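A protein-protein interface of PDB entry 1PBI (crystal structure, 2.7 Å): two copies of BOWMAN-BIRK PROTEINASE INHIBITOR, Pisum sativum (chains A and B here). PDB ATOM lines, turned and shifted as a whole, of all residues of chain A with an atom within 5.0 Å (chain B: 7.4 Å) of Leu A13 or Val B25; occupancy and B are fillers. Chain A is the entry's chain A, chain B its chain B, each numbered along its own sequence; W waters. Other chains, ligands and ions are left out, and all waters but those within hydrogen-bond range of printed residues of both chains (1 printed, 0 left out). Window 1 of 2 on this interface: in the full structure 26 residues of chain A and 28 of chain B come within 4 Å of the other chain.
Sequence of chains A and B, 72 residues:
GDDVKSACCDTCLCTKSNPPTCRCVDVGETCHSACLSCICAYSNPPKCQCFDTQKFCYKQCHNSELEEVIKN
Of the 10 printed residues of chain A, 8 touch a printed residue of chain B.
Along chain A the printed residues that touch a printed residue of chain B span positions 11 to 69.
Of the 21 printed residues of chain B, 12 touch a printed residue of chain A.
Among the printed residues, 23 pairs touch across the chains.
Among the printed residues, Asp or Glu carboxylates within 4 Å of a Lys or Arg side-chain nitrogen of the other chain: Arg A23 with Glu B67.
Among the printed residues, merely in contact across the chains: Thr A15 with Leu B66 (3.1 Å), Cys A14 with Ile B70 (3.2 Å), Arg A23 with Val B27 (3.2 Å), Leu A13 with Glu B67 (3.2 Å), Leu A13 with Val B69 (3.3 Å), Val A69 with Leu B13 (3.3 Å), Cys A14 with Glu B67 (3.4 Å), Cys A12 with Asn B72 (3.5 Å), Leu A13 with Glu B68 (3.5 Å), Cys A12 with Val B69 (3.5 Å), Val A69 with Cys B12 (3.6 Å), Leu A13 with Val B25 (3.6 Å), Thr A15 with Glu B68 (3.7 Å), Val A69 with Val B69 (3.7 Å), Val A25 with Leu B13 (3.8 Å), Cys A12 with Glu B68 (3.9 Å) and Thr A11 with Leu B13 (3.9 Å).
Thr A11 touches Leu B13, but with the chains exchanged Leu A13 does not touch Thr B11 (4.2 Å).
Cys A12 touches Val B69, and with the chains exchanged Val A69 touches Cys B12.
Leu A13 touches Val B25, and with the chains exchanged Val A25 touches Leu B13.
Leu A13 touches Val B69, and with the chains exchanged Val A69 touches Leu B13.
Positions printed for both chains: 11, 12, 13, 23, 25 and 69.
The backbone carbonyl oxygen (O) of Cys A12 sits at hydrogen-bond distance from the backbone NH (N) of Ile B70 (3.0 Å).
The backbone carbonyl oxygen (O) of Cys A14 sits at hydrogen-bond distance from the backbone NH (N) of Glu B68 (2.8 Å).
The backbone carbonyl oxygen of Val B25 sits at hydrogen-bond distance from the guanidinium group of Arg A23 (2.7 Å).
NH1 of Arg A23 sits at hydrogen-bond distance from OE1 of Gln B49.
The guanidinium group (NH2) of Arg A23 is in salt-bridge range of the side-chain carboxylate (OE1) of Glu B67 (3.1 Å).
The backbone carbonyl oxygen (O) of Val A25 is in hydrogen-bond range of the guanidinium group (NH2) of Arg B23, at 2.9 Å.
The backbone carbonyl oxygen (O) of Thr A11 sits at hydrogen-bond distance from the backbone NH (N) of Val A25, 3.1 Å away.
SG of Cys A22 is disulfide-bonded to SG of Cys A14, 2.0 Å away.
The backbone NH of Thr A15 lies within hydrogen-bond range of the backbone carbonyl oxygen of Thr A21 (3.1 Å).
The backbone carbonyl oxygen (O) of Leu B13 lies within hydrogen-bond range of the backbone NH (N) of Arg B23, at 2.9 Å.
The side-chain amide oxygen (OD1) of Asn B72 sits close to the backbone carbonyl oxygen (O) of Ile B70 (3.3 Å).
The side-chain sulfur (SG) of Cys B24 forms a disulfide with the side-chain sulfur (SG) of Cys B9 (2.0 Å).
Of chain B, only Val B25 (3.6 Å), Glu B67 (3.2 Å), Glu B68 (3.5 Å) and Val B69 (3.3 Å) come within 4 Å of Leu A13.
Of the printed residues of chain B, Val A69 touches Cys B12, Leu B13 and Val B69.
Asp B10 touches none of the printed residues of chain A.
Of the printed residues of chain A, Cys B12 touches Val A69.
Of chain A, only Leu A13 and Arg A23 come within 4 Å of Val B25.
Of the printed residues of chain A, Val B27 touches Arg A23 (3.2 Å).
The nearest residue of chain B that does not touch Leu A13 is Thr B11 (4.2 Å).
Water W1 lies within hydrogen-bond range of O of Thr A21 (3.4 Å) and OE2 of Glu B67 (3.4 Å).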
ATOM      1  N   THR A  11      11.224 -35.561  19.616  1.00  0.00           N
ATOM      2  CA  THR A  11      11.670 -34.189  19.841  1.00  0.00           C
ATOM      3  C   THR A  11      11.964 -33.447  18.548  1.00  0.00           C
ATOM      4  O   THR A  11      13.046 -33.540  17.986  1.00  0.00           O
ATOM      5  CB  THR A  11      12.923 -34.160  20.747  1.00  0.00           C
ATOM      6  OG1 THR A  11      12.613 -34.793  22.000  1.00  0.00           O
ATOM      7  CG2 THR A  11      13.379 -32.724  20.996  1.00  0.00           C
ATOM      8  N   CYS A  12      10.977 -32.698  18.088  1.00  0.00           N
ATOM      9  CA  CYS A  12      11.110 -31.923  16.870  1.00  0.00           C
ATOM     10  C   CYS A  12      11.473 -30.479  17.200  1.00  0.00           C
ATOM     11  O   CYS A  12      10.768 -29.805  17.956  1.00  0.00           O
ATOM     12  CB  CYS A  12       9.801 -31.960  16.093  1.00  0.00           C
ATOM     13  SG  CYS A  12       9.915 -31.195  14.455  1.00  0.00           S
ATOM     14  N   LEU A  13      12.571 -30.011  16.617  1.00  0.00           N
ATOM     15  CA  LEU A  13      13.051 -28.657  16.846  1.00  0.00           C
ATOM     16  C   LEU A  13      12.874 -27.805  15.606  1.00  0.00           C
ATOM     17  O   LEU A  13      13.344 -28.168  14.529  1.00  0.00           O
ATOM     18  CB  LEU A  13      14.536 -28.683  17.217  1.00  0.00           C
ATOM     19  CG  LEU A  13      14.952 -28.354  18.649  1.00  0.00           C
ATOM     20  CD1 LEU A  13      14.178 -29.204  19.645  1.00  0.00           C
ATOM     21  CD2 LEU A  13      16.450 -28.601  18.784  1.00  0.00           C
ATOM     22  N   CYS A  14      12.199 -26.672  15.756  1.00  0.00           N
ATOM     23  CA  CYS A  14      11.987 -25.763  14.636  1.00  0.00           C
ATOM     24  C   CYS A  14      12.527 -24.401  15.018  1.00  0.00           C
ATOM     25  O   CYS A  14      12.467 -24.005  16.181  1.00  0.00           O
ATOM     26  CB  CYS A  14      10.491 -25.606  14.303  1.00  0.00           C
ATOM     27  SG  CYS A  14       9.613 -27.065  13.659  1.00  0.00           S
ATOM     28  N   THR A  15      13.051 -23.686  14.030  1.00  0.00           N
ATOM     29  CA  THR A  15      13.561 -22.345  14.257  1.00  0.00           C
ATOM     30  C   THR A  15      12.336 -21.451  14.389  1.00  0.00           C
ATOM     31  O   THR A  15      11.228 -21.843  14.033  1.00  0.00           O
ATOM     32  CB  THR A  15      14.407 -21.837  13.063  1.00  0.00           C
ATOM     33  OG1 THR A  15      13.548 -21.542  11.956  1.00  0.00           O
ATOM     34  CG2 THR A  15      15.422 -22.876  12.643  1.00  0.00           C
ATOM     35  N   THR A  21      12.412 -23.882   9.860  1.00  0.00           N
ATOM     36  CA  THR A  21      13.132 -25.045   9.358  1.00  0.00           C
ATOM     37  C   THR A  21      13.139 -26.009  10.524  1.00  0.00           C
ATOM     38  O   THR A  21      13.450 -25.625  11.650  1.00  0.00           O
ATOM     39  CB  THR A  21      14.570 -24.677   8.960  1.00  0.00           C
ATOM     40  OG1 THR A  21      14.621 -24.442   7.547  1.00  0.00           O
ATOM     41  CG2 THR A  21      15.539 -25.791   9.321  1.00  0.00           C
ATOM     42  N   CYS A  22      12.778 -27.259  10.268  1.00  0.00           N
ATOM     43  CA  CYS A  22      12.718 -28.222  11.347  1.00  0.00           C
ATOM     44  C   CYS A  22      13.565 -29.469  11.162  1.00  0.00           C
ATOM     45  O   CYS A  22      13.960 -29.823  10.043  1.00  0.00           O
ATOM     46  CB  CYS A  22      11.257 -28.603  11.592  1.00  0.00           C
ATOM     47  SG  CYS A  22      10.129 -27.172  11.698  1.00  0.00           S
ATOM     48  N   ARG A  23      13.853 -30.119  12.287  1.00  0.00           N
ATOM     49  CA  ARG A  23      14.645 -31.341  12.302  1.00  0.00           C
ATOM     50  C   ARG A  23      14.224 -32.208  13.481  1.00  0.00           C
ATOM     51  O   ARG A  23      13.534 -31.748  14.387  1.00  0.00           O
ATOM     52  CB  ARG A  23      16.140 -31.019  12.415  1.00  0.00           C
ATOM     53  CG  ARG A  23      16.533 -30.288  13.701  1.00  0.00           C
ATOM     54  CD  ARG A  23      17.975 -29.823  13.681  1.00  0.00           C
ATOM     55  NE  ARG A  23      18.283 -28.997  14.848  1.00  0.00           N
ATOM     56  CZ  ARG A  23      19.294 -29.226  15.687  1.00  0.00           C
ATOM     57  NH1 ARG A  23      20.109 -30.262  15.504  1.00  0.00           N
ATOM     58  NH2 ARG A  23      19.483 -28.420  16.723  1.00  0.00           N
ATOM     59  N   VAL A  25      15.685 -34.317  16.572  1.00  0.00           N
ATOM     60  CA  VAL A  25      16.925 -34.521  17.334  1.00  0.00           C
ATOM     61  C   VAL A  25      16.964 -35.776  18.198  1.00  0.00           C
ATOM     62  O   VAL A  25      17.789 -35.880  19.104  1.00  0.00           O
ATOM     63  CB  VAL A  25      17.271 -33.299  18.225  1.00  0.00           C
ATOM     64  CG1 VAL A  25      17.704 -32.133  17.356  1.00  0.00           C
ATOM     65  CG2 VAL A  25      16.087 -32.911  19.080  1.00  0.00           C
ATOM     66  N   VAL A  69      13.707 -27.833  26.449  1.00  0.00           N
ATOM     67  CA  VAL A  69      14.804 -26.905  26.218  1.00  0.00           C
ATOM     68  C   VAL A  69      15.029 -26.056  27.467  1.00  0.00           C
ATOM     69  O   VAL A  69      14.147 -25.309  27.870  1.00  0.00           O
ATOM     70  CB  VAL A  69      14.495 -25.962  25.033  1.00  0.00           C
ATOM     71  CG1 VAL A  69      15.497 -24.825  24.999  1.00  0.00           C
ATOM     72  CG2 VAL A  69      14.529 -26.737  23.730  1.00  0.00           C
ATOM     73  N   CYS B   9      26.702 -22.934  24.836  1.00  0.00           N
ATOM     74  CA  CYS B   9      25.643 -23.652  24.162  1.00  0.00           C
ATOM     75  C   CYS B   9      24.343 -22.867  24.109  1.00  0.00           C
ATOM     76  O   CYS B   9      23.809 -22.446  25.139  1.00  0.00           O
ATOM     77  CB  CYS B   9      25.404 -24.999  24.832  1.00  0.00           C
ATOM     78  SG  CYS B   9      24.077 -25.925  24.002  1.00  0.00           S
ATOM     79  N   ASP B  10      23.851 -22.678  22.890  1.00  0.00           N
ATOM     80  CA  ASP B  10      22.624 -21.947  22.632  1.00  0.00           C
ATOM     81  C   ASP B  10      21.378 -22.759  22.976  1.00  0.00           C
ATOM     82  O   ASP B  10      20.488 -22.282  23.687  1.00  0.00           O
ATOM     83  CB  ASP B  10      22.563 -21.572  21.158  1.00  0.00           C
ATOM     84  CG  ASP B  10      23.359 -20.340  20.843  1.00  0.00           C
ATOM     85  OD1 ASP B  10      23.144 -19.314  21.522  1.00  0.00           O
ATOM     86  OD2 ASP B  10      24.195 -20.397  19.917  1.00  0.00           O
ATOM     87  N   THR B  11      21.310 -23.983  22.453  1.00  0.00           N
ATOM     88  CA  THR B  11      20.162 -24.863  22.677  1.00  0.00           C
ATOM     89  C   THR B  11      20.548 -26.079  23.496  1.00  0.00           C
ATOM     90  O   THR B  11      21.107 -27.044  22.975  1.00  0.00           O
ATOM     91  CB  THR B  11      19.550 -25.342  21.338  1.00  0.00           C
ATOM     92  OG1 THR B  11      19.262 -24.212  20.506  1.00  0.00           O
ATOM     93  CG2 THR B  11      18.264 -26.112  21.583  1.00  0.00           C
ATOM     94  N   CYS B  12      20.232 -26.024  24.784  1.00  0.00           N
ATOM     95  CA  CYS B  12      20.552 -27.111  25.693  1.00  0.00           C
ATOM     96  C   CYS B  12      19.317 -27.947  25.980  1.00  0.00           C
ATOM     97  O   CYS B  12      18.318 -27.443  26.500  1.00  0.00           O
ATOM     98  CB  CYS B  12      21.117 -26.546  26.992  1.00  0.00           C
ATOM     99  SG  CYS B  12      21.878 -27.771  28.096  1.00  0.00           S
ATOM    100  N   LEU B  13      19.397 -29.228  25.639  1.00  0.00           N
ATOM    101  CA  LEU B  13      18.289 -30.148  25.837  1.00  0.00           C
ATOM    102  C   LEU B  13      18.552 -31.058  27.012  1.00  0.00           C
ATOM    103  O   LEU B  13      19.589 -31.719  27.065  1.00  0.00           O
ATOM    104  CB  LEU B  13      18.093 -31.016  24.593  1.00  0.00           C
ATOM    105  CG  LEU B  13      17.366 -30.494  23.353  1.00  0.00           C
ATOM    106  CD1 LEU B  13      16.799 -31.696  22.609  1.00  0.00           C
ATOM    107  CD2 LEU B  13      16.259 -29.525  23.738  1.00  0.00           C
ATOM    108  N   ARG B  23      22.370 -32.389  26.830  1.00  0.00           N
ATOM    109  CA  ARG B  23      23.237 -32.335  25.671  1.00  0.00           C
ATOM    110  C   ARG B  23      23.016 -31.037  24.920  1.00  0.00           C
ATOM    111  O   ARG B  23      21.985 -30.388  25.080  1.00  0.00           O
ATOM    112  CB  ARG B  23      22.983 -33.536  24.757  1.00  0.00           C
ATOM    113  CG  ARG B  23      21.671 -33.495  24.015  1.00  0.00           C
ATOM    114  CD  ARG B  23      21.347 -34.846  23.383  1.00  0.00           C
ATOM    115  NE  ARG B  23      19.909 -34.957  23.164  1.00  0.00           N
ATOM    116  CZ  ARG B  23      19.338 -35.140  21.979  1.00  0.00           C
ATOM    117  NH1 ARG B  23      20.071 -35.240  20.882  1.00  0.00           N
ATOM    118  NH2 ARG B  23      18.023 -35.193  21.894  1.00  0.00           N
ATOM    119  N   CYS B  24      23.999 -30.649  24.119  1.00  0.00           N
ATOM    120  CA  CYS B  24      23.902 -29.425  23.351  1.00  0.00           C
ATOM    121  C   CYS B  24      23.644 -29.811  21.911  1.00  0.00           C
ATOM    122  O   CYS B  24      24.493 -30.454  21.284  1.00  0.00           O
ATOM    123  CB  CYS B  24      25.201 -28.644  23.432  1.00  0.00           C
ATOM    124  SG  CYS B  24      25.073 -27.026  22.622  1.00  0.00           S
ATOM    125  N   VAL B  25      22.485 -29.419  21.382  1.00  0.00           N
ATOM    126  CA  VAL B  25      22.115 -29.776  20.016  1.00  0.00           C
ATOM    127  C   VAL B  25      22.429 -28.707  18.972  1.00  0.00           C
ATOM    128  O   VAL B  25      21.846 -28.695  17.896  1.00  0.00           O
ATOM    129  CB  VAL B  25      20.613 -30.154  19.933  1.00  0.00           C
ATOM    130  CG1 VAL B  25      20.291 -31.191  20.969  1.00  0.00           C
ATOM    131  CG2 VAL B  25      19.747 -28.940  20.137  1.00  0.00           C
ATOM    132  N   ASP B  26      23.365 -27.824  19.279  1.00  0.00           N
ATOM    133  CA  ASP B  26      23.733 -26.778  18.342  1.00  0.00           C
ATOM    134  C   ASP B  26      24.416 -27.433  17.147  1.00  0.00           C
ATOM    135  O   ASP B  26      25.135 -28.416  17.306  1.00  0.00           O
ATOM    136  CB  ASP B  26      24.698 -25.785  19.004  1.00  0.00           C
ATOM    137  CG  ASP B  26      23.997 -24.788  19.919  1.00  0.00           C
ATOM    138  OD1 ASP B  26      22.750 -24.842  20.043  1.00  0.00           O
ATOM    139  OD2 ASP B  26      24.704 -23.947  20.519  1.00  0.00           O
ATOM    140  N   VAL B  27      24.182 -26.882  15.956  1.00  0.00           N
ATOM    141  CA  VAL B  27      24.778 -27.397  14.720  1.00  0.00           C
ATOM    142  C   VAL B  27      25.655 -26.321  14.074  1.00  0.00           C
ATOM    143  O   VAL B  27      25.363 -25.131  14.190  1.00  0.00           O
ATOM    144  CB  VAL B  27      23.698 -27.784  13.683  1.00  0.00           C
ATOM    145  CG1 VAL B  27      24.285 -28.717  12.655  1.00  0.00           C
ATOM    146  CG2 VAL B  27      22.513 -28.401  14.371  1.00  0.00           C
ATOM    147  N   GLY B  28      26.714 -26.735  13.380  1.00  0.00           N
ATOM    148  CA  GLY B  28      27.578 -25.767  12.726  1.00  0.00           C
ATOM    149  C   GLY B  28      28.782 -26.389  12.059  1.00  0.00           C
ATOM    150  O   GLY B  28      28.911 -27.609  12.019  1.00  0.00           O
ATOM    151  N   CYS B  48      28.019 -30.072  11.961  1.00  0.00           N
ATOM    152  CA  CYS B  48      28.480 -30.822  13.125  1.00  0.00           C
ATOM    153  C   CYS B  48      27.662 -30.577  14.367  1.00  0.00           C
ATOM    154  O   CYS B  48      27.123 -29.495  14.585  1.00  0.00           O
ATOM    155  CB  CYS B  48      29.930 -30.492  13.441  1.00  0.00           C
ATOM    156  SG  CYS B  48      31.040 -30.526  12.012  1.00  0.00           S
ATOM    157  N   GLN B  49      27.571 -31.607  15.187  1.00  0.00           N
ATOM    158  CA  GLN B  49      26.839 -31.504  16.428  1.00  0.00           C
ATOM    159  C   GLN B  49      27.614 -32.275  17.474  1.00  0.00           C
ATOM    160  O   GLN B  49      28.251 -33.284  17.173  1.00  0.00           O
ATOM    161  CB  GLN B  49      25.436 -32.084  16.291  1.00  0.00           C
ATOM    162  CG  GLN B  49      24.557 -31.661  17.421  1.00  0.00           C
ATOM    163  CD  GLN B  49      23.232 -32.354  17.421  1.00  0.00           C
ATOM    164  OE1 GLN B  49      22.367 -32.025  16.624  1.00  0.00           O
ATOM    165  NE2 GLN B  49      23.057 -33.319  18.319  1.00  0.00           N
ATOM    166  N   CYS B  50      27.569 -31.781  18.703  1.00  0.00           N
ATOM    167  CA  CYS B  50      28.275 -32.403  19.807  1.00  0.00           C
ATOM    168  C   CYS B  50      27.397 -33.465  20.434  1.00  0.00           C
ATOM    169  O   CYS B  50      26.331 -33.160  20.969  1.00  0.00           O
ATOM    170  CB  CYS B  50      28.637 -31.351  20.850  1.00  0.00           C
ATOM    171  SG  CYS B  50      29.728 -32.012  22.139  1.00  0.00           S
ATOM    172  N   ASP B  52      28.131 -35.240  23.058  1.00  0.00           N
ATOM    173  CA  ASP B  52      28.399 -35.369  24.490  1.00  0.00           C
ATOM    174  C   ASP B  52      27.122 -35.267  25.305  1.00  0.00           C
ATOM    175  O   ASP B  52      26.156 -34.645  24.887  1.00  0.00           O
ATOM    176  CB  ASP B  52      29.368 -34.282  24.959  1.00  0.00           C
ATOM    177  CG  ASP B  52      30.762 -34.454  24.400  1.00  0.00           C
ATOM    178  OD1 ASP B  52      31.159 -35.593  24.077  1.00  0.00           O
ATOM    179  OD2 ASP B  52      31.466 -33.438  24.279  1.00  0.00           O
ATOM    180  N   LEU B  66      17.053 -19.413  19.020  1.00  0.00           N
ATOM    181  CA  LEU B  66      16.822 -19.549  17.591  1.00  0.00           C
ATOM    182  C   LEU B  66      16.023 -20.800  17.258  1.00  0.00           C
ATOM    183  O   LEU B  66      15.683 -21.037  16.098  1.00  0.00           O
ATOM    184  CB  LEU B  66      18.157 -19.591  16.839  1.00  0.00           C
ATOM    185  CG  LEU B  66      19.388 -20.131  17.573  1.00  0.00           C
ATOM    186  CD1 LEU B  66      19.081 -21.469  18.228  1.00  0.00           C
ATOM    187  CD2 LEU B  66      20.528 -20.271  16.579  1.00  0.00           C
ATOM    188  N   GLU B  67      15.725 -21.601  18.274  1.00  0.00           N
ATOM    189  CA  GLU B  67      14.977 -22.828  18.062  1.00  0.00           C
ATOM    190  C   GLU B  67      14.063 -23.125  19.236  1.00  0.00           C
ATOM    191  O   GLU B  67      14.353 -22.751  20.373  1.00  0.00           O
ATOM    192  CB  GLU B  67      15.933 -24.001  17.839  1.00  0.00           C
ATOM    193  CG  GLU B  67      16.526 -24.056  16.438  1.00  0.00           C
ATOM    194  CD  GLU B  67      17.251 -25.355  16.169  1.00  0.00           C
ATOM    195  OE1 GLU B  67      17.610 -26.047  17.143  1.00  0.00           O
ATOM    196  OE2 GLU B  67      17.460 -25.687  14.986  1.00  0.00           O
ATOM    197  N   GLU B  68      12.951 -23.796  18.945  1.00  0.00           N
ATOM    198  CA  GLU B  68      11.964 -24.152  19.956  1.00  0.00           C
ATOM    199  C   GLU B  68      11.460 -25.563  19.707  1.00  0.00           C
ATOM    200  O   GLU B  68      11.475 -26.041  18.577  1.00  0.00           O
ATOM    201  CB  GLU B  68      10.783 -23.174  19.910  1.00  0.00           C
ATOM    202  CG  GLU B  68      10.712 -22.335  18.628  1.00  0.00           C
ATOM    203  CD  GLU B  68       9.283 -22.007  18.198  1.00  0.00           C
ATOM    204  OE1 GLU B  68       8.427 -21.769  19.082  1.00  0.00           O
ATOM    205  OE2 GLU B  68       9.018 -21.986  16.971  1.00  0.00           O
ATOM    206  N   VAL B  69      11.024 -26.225  20.768  1.00  0.00           N
ATOM    207  CA  VAL B  69      10.502 -27.574  20.658  1.00  0.00           C
ATOM    208  C   VAL B  69       9.024 -27.492  20.298  1.00  0.00           C
ATOM    209  O   VAL B  69       8.229 -26.921  21.043  1.00  0.00           O
ATOM    210  CB  VAL B  69      10.653 -28.351  21.985  1.00  0.00           C
ATOM    211  CG1 VAL B  69       9.606 -29.456  22.066  1.00  0.00           C
ATOM    212  CG2 VAL B  69      12.048 -28.943  22.088  1.00  0.00           C
ATOM    213  N   ILE B  70       8.663 -28.060  19.150  1.00  0.00           N
ATOM    214  CA  ILE B  70       7.278 -28.059  18.697  1.00  0.00           C
ATOM    215  C   ILE B  70       6.538 -29.291  19.203  1.00  0.00           C
ATOM    216  O   ILE B  70       6.875 -30.413  18.837  1.00  0.00           O
ATOM    217  CB  ILE B  70       7.208 -28.056  17.182  1.00  0.00           C
ATOM    218  CG1 ILE B  70       8.329 -27.174  16.617  1.00  0.00           C
ATOM    219  CG2 ILE B  70       5.823 -27.626  16.738  1.00  0.00           C
ATOM    220  CD1 ILE B  70       7.899 -25.791  16.211  1.00  0.00           C
ATOM    221  N   ASN B  72       4.604 -31.752  18.763  1.00  0.00           N
ATOM    222  CA  ASN B  72       4.006 -32.480  17.644  1.00  0.00           C
ATOM    223  C   ASN B  72       3.309 -33.746  18.133  1.00  0.00           C
ATOM    224  O   ASN B  72       2.456 -33.642  19.039  1.00  0.00           O
ATOM    225  CB  ASN B  72       5.095 -32.860  16.636  1.00  0.00           C
ATOM    226  CG  ASN B  72       6.263 -33.598  17.288  1.00  0.00           C
ATOM    227  OD1 ASN B  72       6.367 -33.665  18.514  1.00  0.00           O
ATOM    228  ND2 ASN B  72       7.142 -34.158  16.467  1.00  0.00           N
HETATM  229  O   HOH W   1      16.711 -26.491  11.786  1.00  0.00           O
